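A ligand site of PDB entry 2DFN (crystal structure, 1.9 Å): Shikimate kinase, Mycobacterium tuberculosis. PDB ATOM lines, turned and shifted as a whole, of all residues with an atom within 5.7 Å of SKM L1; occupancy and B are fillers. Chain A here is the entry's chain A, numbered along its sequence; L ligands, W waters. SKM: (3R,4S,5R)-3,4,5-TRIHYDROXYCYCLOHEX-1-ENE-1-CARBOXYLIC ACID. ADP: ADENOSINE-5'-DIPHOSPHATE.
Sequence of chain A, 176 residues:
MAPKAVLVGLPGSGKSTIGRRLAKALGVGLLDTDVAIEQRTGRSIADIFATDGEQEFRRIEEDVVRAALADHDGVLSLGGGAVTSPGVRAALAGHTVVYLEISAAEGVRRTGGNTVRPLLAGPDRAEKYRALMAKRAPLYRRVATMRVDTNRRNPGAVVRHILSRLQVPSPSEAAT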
ATOM      1  N   PRO A  11      -4.651 -20.766 -20.894  1.00  0.00           N
ATOM      2  CA  PRO A  11      -4.548 -20.239 -19.537  1.00  0.00           C
ATOM      3  C   PRO A  11      -3.931 -21.300 -18.645  1.00  0.00           C
ATOM      4  O   PRO A  11      -4.242 -22.483 -18.779  1.00  0.00           O
ATOM      5  CB  PRO A  11      -6.002 -20.075 -19.114  1.00  0.00           C
ATOM      6  CG  PRO A  11      -6.831 -20.490 -20.303  1.00  0.00           C
ATOM      7  CD  PRO A  11      -5.986 -20.657 -21.482  1.00  0.00           C
ATOM      8  N   LYS A  15       2.533 -19.161 -19.457  1.00  0.00           N
ATOM      9  CA  LYS A  15       2.985 -17.975 -20.276  1.00  0.00           C
ATOM     10  C   LYS A  15       3.636 -16.886 -19.396  1.00  0.00           C
ATOM     11  O   LYS A  15       4.743 -16.376 -19.680  1.00  0.00           O
ATOM     12  CB  LYS A  15       1.823 -17.333 -21.112  1.00  0.00           C
ATOM     13  CG  LYS A  15       1.318 -18.254 -22.267  1.00  0.00           C
ATOM     14  CD  LYS A  15       0.098 -17.670 -23.058  1.00  0.00           C
ATOM     15  CE  LYS A  15      -1.025 -17.197 -22.141  1.00  0.00           C
ATOM     16  NZ  LYS A  15      -1.575 -18.284 -21.237  1.00  0.00           N
ATOM     17  N   ASP A  34      -1.312  -9.182 -21.244  1.00  0.00           N
ATOM     18  CA  ASP A  34      -2.442  -9.084 -20.317  1.00  0.00           C
ATOM     19  C   ASP A  34      -2.217  -7.890 -19.391  1.00  0.00           C
ATOM     20  O   ASP A  34      -3.135  -7.075 -19.159  1.00  0.00           O
ATOM     21  CB  ASP A  34      -2.535 -10.355 -19.450  1.00  0.00           C
ATOM     22  CG  ASP A  34      -3.399 -11.453 -20.082  1.00  0.00           C
ATOM     23  OD1 ASP A  34      -4.040 -11.210 -21.135  1.00  0.00           O
ATOM     24  OD2 ASP A  34      -3.430 -12.564 -19.520  1.00  0.00           O
ATOM     25  N   ILE A  45      -8.893  -7.062 -16.612  1.00  0.00           N
ATOM     26  CA  ILE A  45      -9.256  -7.875 -17.770  1.00  0.00           C
ATOM     27  C   ILE A  45     -10.700  -8.301 -17.573  1.00  0.00           C
ATOM     28  O   ILE A  45     -11.483  -8.332 -18.529  1.00  0.00           O
ATOM     29  CB  ILE A  45      -8.324  -9.112 -17.894  1.00  0.00           C
ATOM     30  CG1 ILE A  45      -6.937  -8.645 -18.293  1.00  0.00           C
ATOM     31  CG2 ILE A  45      -8.918 -10.165 -18.829  1.00  0.00           C
ATOM     32  CD1 ILE A  45      -7.012  -7.357 -19.101  1.00  0.00           C
ATOM     33  N   PHE A  49     -13.908  -7.569 -20.069  1.00  0.00           N
ATOM     34  CA  PHE A  49     -14.758  -8.646 -20.565  1.00  0.00           C
ATOM     35  C   PHE A  49     -16.232  -8.392 -20.166  1.00  0.00           C
ATOM     36  O   PHE A  49     -17.158  -8.776 -20.904  1.00  0.00           O
ATOM     37  CB  PHE A  49     -14.287 -10.016 -20.060  1.00  0.00           C
ATOM     38  CG  PHE A  49     -13.387 -10.758 -21.040  1.00  0.00           C
ATOM     39  CD1 PHE A  49     -13.844 -11.893 -21.709  1.00  0.00           C
ATOM     40  CD2 PHE A  49     -12.072 -10.344 -21.259  1.00  0.00           C
ATOM     41  CE1 PHE A  49     -13.017 -12.584 -22.594  1.00  0.00           C
ATOM     42  CE2 PHE A  49     -11.225 -11.038 -22.131  1.00  0.00           C
ATOM     43  CZ  PHE A  49     -11.711 -12.161 -22.820  1.00  0.00           C
ATOM     44  N   GLU A  54     -15.700  -9.575 -24.836  1.00  0.00           N
ATOM     45  CA  GLU A  54     -14.578 -10.217 -25.506  1.00  0.00           C
ATOM     46  C   GLU A  54     -14.132  -9.596 -26.837  1.00  0.00           C
ATOM     47  O   GLU A  54     -12.939  -9.417 -27.063  1.00  0.00           O
ATOM     48  CB  GLU A  54     -14.883 -11.703 -25.700  1.00  0.00           C
ATOM     49  CG  GLU A  54     -13.712 -12.646 -25.487  1.00  0.00           C
ATOM     50  CD  GLU A  54     -13.299 -13.366 -26.754  1.00  0.00           C
ATOM     51  OE1 GLU A  54     -13.507 -12.788 -27.841  1.00  0.00           O
ATOM     52  OE2 GLU A  54     -12.757 -14.507 -26.664  1.00  0.00           O
ATOM     53  N   PHE A  57     -12.140  -6.507 -25.899  1.00  0.00           N
ATOM     54  CA  PHE A  57     -10.841  -6.993 -25.409  1.00  0.00           C
ATOM     55  C   PHE A  57      -9.934  -7.430 -26.551  1.00  0.00           C
ATOM     56  O   PHE A  57      -8.774  -7.001 -26.620  1.00  0.00           O
ATOM     57  CB  PHE A  57     -11.009  -8.185 -24.467  1.00  0.00           C
ATOM     58  CG  PHE A  57      -9.705  -8.729 -23.969  1.00  0.00           C
ATOM     59  CD1 PHE A  57      -9.011  -8.060 -22.970  1.00  0.00           C
ATOM     60  CD2 PHE A  57      -9.158  -9.895 -24.519  1.00  0.00           C
ATOM     61  CE1 PHE A  57      -7.791  -8.566 -22.491  1.00  0.00           C
ATOM     62  CE2 PHE A  57      -7.957 -10.412 -24.042  1.00  0.00           C
ATOM     63  CZ  PHE A  57      -7.255  -9.752 -23.036  1.00  0.00           C
ATOM     64  N   ARG A  58     -10.462  -8.291 -27.436  1.00  0.00           N
ATOM     65  CA  ARG A  58      -9.687  -8.872 -28.547  1.00  0.00           C
ATOM     66  C   ARG A  58      -9.125  -7.780 -29.445  1.00  0.00           C
ATOM     67  O   ARG A  58      -7.968  -7.833 -29.875  1.00  0.00           O
ATOM     68  CB  ARG A  58     -10.506  -9.843 -29.390  1.00  0.00           C
ATOM     69  CG  ARG A  58     -10.972 -11.092 -28.684  1.00  0.00           C
ATOM     70  CD  ARG A  58      -9.826 -11.908 -28.092  1.00  0.00           C
ATOM     71  NE  ARG A  58     -10.311 -12.919 -27.149  1.00  0.00           N
ATOM     72  CZ  ARG A  58      -9.573 -13.464 -26.181  1.00  0.00           C
ATOM     73  NH1 ARG A  58      -8.290 -13.110 -26.042  1.00  0.00           N
ATOM     74  NH2 ARG A  58     -10.089 -14.368 -25.354  1.00  0.00           N
ATOM     75  N   GLU A  61      -6.343  -5.986 -27.364  1.00  0.00           N
ATOM     76  CA  GLU A  61      -5.288  -6.976 -27.330  1.00  0.00           C
ATOM     77  C   GLU A  61      -4.460  -7.040 -28.631  1.00  0.00           C
ATOM     78  O   GLU A  61      -3.211  -6.982 -28.578  1.00  0.00           O
ATOM     79  CB  GLU A  61      -5.885  -8.330 -26.939  1.00  0.00           C
ATOM     80  CG  GLU A  61      -4.870  -9.458 -26.924  1.00  0.00           C
ATOM     81  CD  GLU A  61      -5.502 -10.797 -26.529  1.00  0.00           C
ATOM     82  OE1 GLU A  61      -6.411 -11.278 -27.265  1.00  0.00           O
ATOM     83  OE2 GLU A  61      -5.042 -11.366 -25.502  1.00  0.00           O
ATOM     84  N   LEU A  78       1.737 -13.594 -24.558  1.00  0.00           N
ATOM     85  CA  LEU A  78       0.435 -13.191 -25.102  1.00  0.00           C
ATOM     86  C   LEU A  78      -0.664 -13.659 -24.118  1.00  0.00           C
ATOM     87  O   LEU A  78      -0.510 -14.655 -23.436  1.00  0.00           O
ATOM     88  CB  LEU A  78       0.269 -13.886 -26.457  1.00  0.00           C
ATOM     89  CG  LEU A  78       0.552 -13.051 -27.697  1.00  0.00           C
ATOM     90  CD1 LEU A  78       1.759 -12.152 -27.543  1.00  0.00           C
ATOM     91  CD2 LEU A  78       0.460 -13.783 -29.061  1.00  0.00           C
ATOM     92  N   GLY A  79      -1.769 -12.933 -24.026  1.00  0.00           N
ATOM     93  CA  GLY A  79      -3.001 -13.467 -23.421  1.00  0.00           C
ATOM     94  C   GLY A  79      -3.403 -14.805 -24.049  1.00  0.00           C
ATOM     95  O   GLY A  79      -3.073 -15.094 -25.192  1.00  0.00           O
ATOM     96  N   GLY A  80      -3.990 -15.683 -23.258  1.00  0.00           N
ATOM     97  CA  GLY A  80      -4.274 -17.052 -23.675  1.00  0.00           C
ATOM     98  C   GLY A  80      -5.112 -17.217 -24.934  1.00  0.00           C
ATOM     99  O   GLY A  80      -4.973 -18.222 -25.617  1.00  0.00           O
ATOM    100  N   GLY A  81      -5.964 -16.231 -25.233  1.00  0.00           N
ATOM    101  CA  GLY A  81      -6.831 -16.310 -26.382  1.00  0.00           C
ATOM    102  C   GLY A  81      -6.457 -15.316 -27.474  1.00  0.00           C
ATOM    103  O   GLY A  81      -7.252 -15.067 -28.389  1.00  0.00           O
ATOM    104  N   ALA A  82      -5.259 -14.739 -27.385  1.00  0.00           N
ATOM    105  CA  ALA A  82      -4.819 -13.821 -28.440  1.00  0.00           C
ATOM    106  C   ALA A  82      -4.788 -14.506 -29.800  1.00  0.00           C
ATOM    107  O   ALA A  82      -5.094 -13.873 -30.813  1.00  0.00           O
ATOM    108  CB  ALA A  82      -3.418 -13.204 -28.130  1.00  0.00           C
ATOM    109  N   VAL A 116      -8.815 -14.636 -11.683  1.00  0.00           N
ATOM    110  CA  VAL A 116      -9.655 -13.887 -12.617  1.00  0.00           C
ATOM    111  C   VAL A 116     -10.245 -14.807 -13.694  1.00  0.00           C
ATOM    112  O   VAL A 116     -11.368 -15.317 -13.543  1.00  0.00           O
ATOM    113  CB  VAL A 116      -8.887 -12.744 -13.329  1.00  0.00           C
ATOM    114  CG1 VAL A 116      -8.887 -12.950 -14.865  1.00  0.00           C
ATOM    115  CG2 VAL A 116      -9.474 -11.393 -12.945  1.00  0.00           C
ATOM    116  N   ARG A 117      -9.479 -15.000 -14.765  1.00  0.00           N
ATOM    117  CA  ARG A 117      -9.934 -15.620 -16.012  1.00  0.00           C
ATOM    118  C   ARG A 117     -11.428 -15.649 -16.374  1.00  0.00           C
ATOM    119  O   ARG A 117     -12.101 -16.660 -16.154  1.00  0.00           O
ATOM    120  CB  ARG A 117      -9.175 -16.919 -16.293  1.00  0.00           C
ATOM    121  CG  ARG A 117      -7.668 -16.680 -16.592  1.00  0.00           C
ATOM    122  CD  ARG A 117      -6.896 -17.971 -16.825  1.00  0.00           C
ATOM    123  NE  ARG A 117      -5.443 -17.929 -16.607  1.00  0.00           N
ATOM    124  CZ  ARG A 117      -4.839 -18.319 -15.486  1.00  0.00           C
ATOM    125  NH1 ARG A 117      -5.571 -18.706 -14.436  1.00  0.00           N
ATOM    126  NH2 ARG A 117      -3.502 -18.269 -15.384  1.00  0.00           N
ATOM    127  N   PRO A 118     -11.954 -14.547 -16.936  1.00  0.00           N
ATOM    128  CA  PRO A 118     -13.351 -14.536 -17.370  1.00  0.00           C
ATOM    129  C   PRO A 118     -13.830 -15.820 -18.064  1.00  0.00           C
ATOM    130  O   PRO A 118     -14.958 -16.258 -17.835  1.00  0.00           O
ATOM    131  CB  PRO A 118     -13.431 -13.320 -18.285  1.00  0.00           C
ATOM    132  CG  PRO A 118     -12.426 -12.368 -17.681  1.00  0.00           C
ATOM    133  CD  PRO A 118     -11.308 -13.236 -17.185  1.00  0.00           C
ATOM    134  N   LEU A 119     -12.993 -16.423 -18.898  1.00  0.00           N
ATOM    135  CA  LEU A 119     -13.451 -17.518 -19.727  1.00  0.00           C
ATOM    136  C   LEU A 119     -13.415 -18.861 -18.980  1.00  0.00           C
ATOM    137  O   LEU A 119     -14.065 -19.834 -19.373  1.00  0.00           O
ATOM    138  CB  LEU A 119     -12.675 -17.545 -21.060  1.00  0.00           C
ATOM    139  CG  LEU A 119     -13.166 -16.705 -22.244  1.00  0.00           C
ATOM    140  CD1 LEU A 119     -14.479 -15.960 -22.002  1.00  0.00           C
ATOM    141  CD2 LEU A 119     -12.140 -15.831 -22.934  1.00  0.00           C
ATOM    142  N   LEU A 132     -12.110 -24.807 -24.439  1.00  0.00           N
ATOM    143  CA  LEU A 132     -11.011 -23.910 -24.813  1.00  0.00           C
ATOM    144  C   LEU A 132      -9.857 -24.650 -25.541  1.00  0.00           C
ATOM    145  O   LEU A 132      -9.380 -24.224 -26.584  1.00  0.00           O
ATOM    146  CB  LEU A 132     -10.513 -23.294 -23.497  1.00  0.00           C
ATOM    147  CG  LEU A 132     -10.470 -21.781 -23.369  1.00  0.00           C
ATOM    148  CD1 LEU A 132     -11.740 -21.196 -23.902  1.00  0.00           C
ATOM    149  CD2 LEU A 132     -10.186 -21.366 -21.946  1.00  0.00           C
ATOM    150  N   ARG A 136      -8.717 -24.014 -29.359  1.00  0.00           N
ATOM    151  CA  ARG A 136      -7.474 -23.284 -29.534  1.00  0.00           C
ATOM    152  C   ARG A 136      -6.238 -24.085 -29.875  1.00  0.00           C
ATOM    153  O   ARG A 136      -5.309 -23.537 -30.443  1.00  0.00           O
ATOM    154  CB  ARG A 136      -7.178 -22.389 -28.338  1.00  0.00           C
ATOM    155  CG  ARG A 136      -8.383 -21.867 -27.667  1.00  0.00           C
ATOM    156  CD  ARG A 136      -8.331 -20.401 -27.565  1.00  0.00           C
ATOM    157  NE  ARG A 136      -8.817 -19.903 -26.291  1.00  0.00           N
ATOM    158  CZ  ARG A 136      -9.368 -18.702 -26.172  1.00  0.00           C
ATOM    159  NH1 ARG A 136      -9.465 -17.951 -27.258  1.00  0.00           N
ATOM    160  NH2 ARG A 136      -9.817 -18.250 -25.011  1.00  0.00           N
ATOM    161  N   TYR A 140      -2.866 -22.685 -31.690  1.00  0.00           N
ATOM    162  CA  TYR A 140      -1.503 -22.662 -31.091  1.00  0.00           C
ATOM    163  C   TYR A 140      -0.518 -23.409 -31.998  1.00  0.00           C
ATOM    164  O   TYR A 140       0.583 -22.931 -32.259  1.00  0.00           O
ATOM    165  CB  TYR A 140      -1.488 -23.240 -29.656  1.00  0.00           C
ATOM    166  CG  TYR A 140      -2.353 -22.531 -28.646  1.00  0.00           C
ATOM    167  CD1 TYR A 140      -2.206 -21.176 -28.400  1.00  0.00           C
ATOM    168  CD2 TYR A 140      -3.299 -23.244 -27.890  1.00  0.00           C
ATOM    169  CE1 TYR A 140      -2.978 -20.513 -27.462  1.00  0.00           C
ATOM    170  CE2 TYR A 140      -4.067 -22.581 -26.942  1.00  0.00           C
ATOM    171  CZ  TYR A 140      -3.876 -21.243 -26.714  1.00  0.00           C
ATOM    172  OH  TYR A 140      -4.673 -20.522 -25.830  1.00  0.00           O
HETATM  173  O12 SKM L   1      -6.010 -12.519 -21.728  1.00  0.00           O
HETATM  174  C8  SKM L   1      -6.491 -13.211 -20.578  1.00  0.00           C
HETATM  175  C6  SKM L   1      -5.902 -14.636 -20.477  1.00  0.00           C
HETATM  176  O7  SKM L   1      -4.457 -14.826 -20.584  1.00  0.00           O
HETATM  177  C5  SKM L   1      -6.872 -15.691 -21.011  1.00  0.00           C
HETATM  178  C4  SKM L   1      -7.812 -15.420 -21.932  1.00  0.00           C
HETATM  179  C1  SKM L   1      -8.273 -16.357 -22.780  1.00  0.00           C
HETATM  180  O2  SKM L   1      -9.084 -15.985 -23.654  1.00  0.00           O
HETATM  181  O3  SKM L   1      -7.934 -17.551 -22.716  1.00  0.00           O
HETATM  182  C10 SKM L   1      -8.253 -14.140 -22.008  1.00  0.00           C
HETATM  183  C9  SKM L   1      -8.013 -13.260 -20.788  1.00  0.00           C
HETATM  184  O11 SKM L   1      -8.682 -13.716 -19.602  1.00  0.00           O
HETATM  185  PB  ADP L   2      -0.611 -18.385 -18.013  1.00  0.00           P
HETATM  186  O1B ADP L   2      -0.339 -19.202 -19.224  1.00  0.00           O
HETATM  187  O2B ADP L   2       0.198 -17.125 -18.103  1.00  0.00           O
HETATM  188  O3B ADP L   2      -2.059 -18.237 -17.604  1.00  0.00           O
HETATM  189  PA  ADP L   2       0.784 -18.783 -15.476  1.00  0.00           P
HETATM  190  O1A ADP L   2      -0.067 -17.761 -14.782  1.00  0.00           O
HETATM  191  O2A ADP L   2       2.219 -18.493 -15.767  1.00  0.00           O
HETATM  192  O3A ADP L   2       0.034 -19.291 -16.817  1.00  0.00           O
HETATM  193  O5' ADP L   2       0.856 -20.155 -14.624  1.00  0.00           O
HETATM  194  C5' ADP L   2      -0.290 -20.633 -13.902  1.00  0.00           C
HETATM  195  C4' ADP L   2       0.154 -21.280 -12.600  1.00  0.00           C
HETATM  196  O4' ADP L   2       0.734 -22.526 -12.948  1.00  0.00           O
HETATM  197  C3' ADP L   2       1.198 -20.455 -11.829  1.00  0.00           C
HETATM  198  O3' ADP L   2       1.058 -20.597 -10.412  1.00  0.00           O
HETATM  199  C2' ADP L   2       2.515 -21.125 -12.125  1.00  0.00           C
HETATM  200  O2' ADP L   2       3.208 -21.076 -10.885  1.00  0.00           O
HETATM  201  C1' ADP L   2       2.087 -22.555 -12.496  1.00  0.00           C
HETATM  202  N9  ADP L   2       2.977 -23.131 -13.503  1.00  0.00           N
HETATM  203  C8  ADP L   2       3.330 -22.558 -14.667  1.00  0.00           C
HETATM  204  N7  ADP L   2       4.130 -23.388 -15.348  1.00  0.00           N
HETATM  205  C5  ADP L   2       4.358 -24.463 -14.557  1.00  0.00           C
HETATM  206  C6  ADP L   2       5.178 -25.697 -14.668  1.00  0.00           C
HETATM  207  N6  ADP L   2       5.987 -26.005 -15.703  1.00  0.00           N
HETATM  208  N1  ADP L   2       5.095 -26.566 -13.628  1.00  0.00           N
HETATM  209  C2  ADP L   2       4.384 -26.274 -12.535  1.00  0.00           C
HETATM  210  N3  ADP L   2       3.550 -25.234 -12.345  1.00  0.00           N
HETATM  211  C4  ADP L   2       3.560 -24.302 -13.333  1.00  0.00           C
HETATM  212  O   HOH W   1     -10.346 -15.877 -19.400  1.00  0.00           O
HETATM  213  O   HOH W   2      -9.128 -18.236 -20.010  1.00  0.00           O
HETATM  214  O   HOH W   3      -6.096 -13.651 -24.276  1.00  0.00           O
HETATM  215  O   HOH W   4      -3.967 -15.472 -17.248  1.00  0.00           O
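Water W1 lies within hydrogen-bond range of O11 of SKM L1 (2.7 Å) and N of Leu 119 (2.7 Å).
Water W4 lies within hydrogen-bond range of NE of Arg 117 (2.9 Å), O3B of ADP L2 (3.4 Å) and O7 of SKM L1 (3.4 Å).
NH2 of Arg 117 lies within salt-bridge range of O3B of ADP L2 (2.6 Å).
An oxygen (O2) of SKM L1 lies within salt-bridge range of the guanidinium group (NH2) of Arg 136, 2.7 Å away.
An oxygen (O3) of SKM L1 lies close to the backbone NH (N) of Gly 81, 3.5 Å away.
O1B of ADP L2 is in hydrogen-bond range of N of Lys 15, at 2.9 Å.
The side-chain amino group (NZ) of Lys 15 lies within salt-bridge range of an oxygen (O1B) of ADP L2, at 2.5 Å.
An oxygen (O12) of SKM L1 sits at hydrogen-bond distance from the side-chain carboxylate (OD1) of Asp 34, at 2.4 Å.
The guanidinium group of Arg 58 is in salt-bridge range of an oxygen (O2) of SKM L1.
O7 of SKM L1 is in hydrogen-bond range of N of Gly 80, at 2.8 Å.
Merely in contact with SKM L1: Pro 11 (3.9 Å), Ile 45 (3.6 Å), Phe 57 (3.3 Å), Gly 79 (3.5 Å), Pro 118 (3.6 Å) and Leu 119 (3.1 Å).
Hydrophobic or aromatic side chains within 4 Å of SKM L1: Pro 11, Ile 45, Phe 57, Pro 118 and Leu 119.
Of the 21 residues printed, 11 come within 4 Å of SKM L1.
The guanidinium group (NE) of Arg 58 lies within salt-bridge range of the side-chain carboxylate (OE2) of Glu 54 (3.0 Å).
NH1 of Arg 58 is in salt-bridge range of OE1 of Glu 61, 2.9 Å away.
The backbone carbonyl oxygen (O) of Gly 81 sits close to the guanidinium group (NH1) of Arg 58 (3.2 Å).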
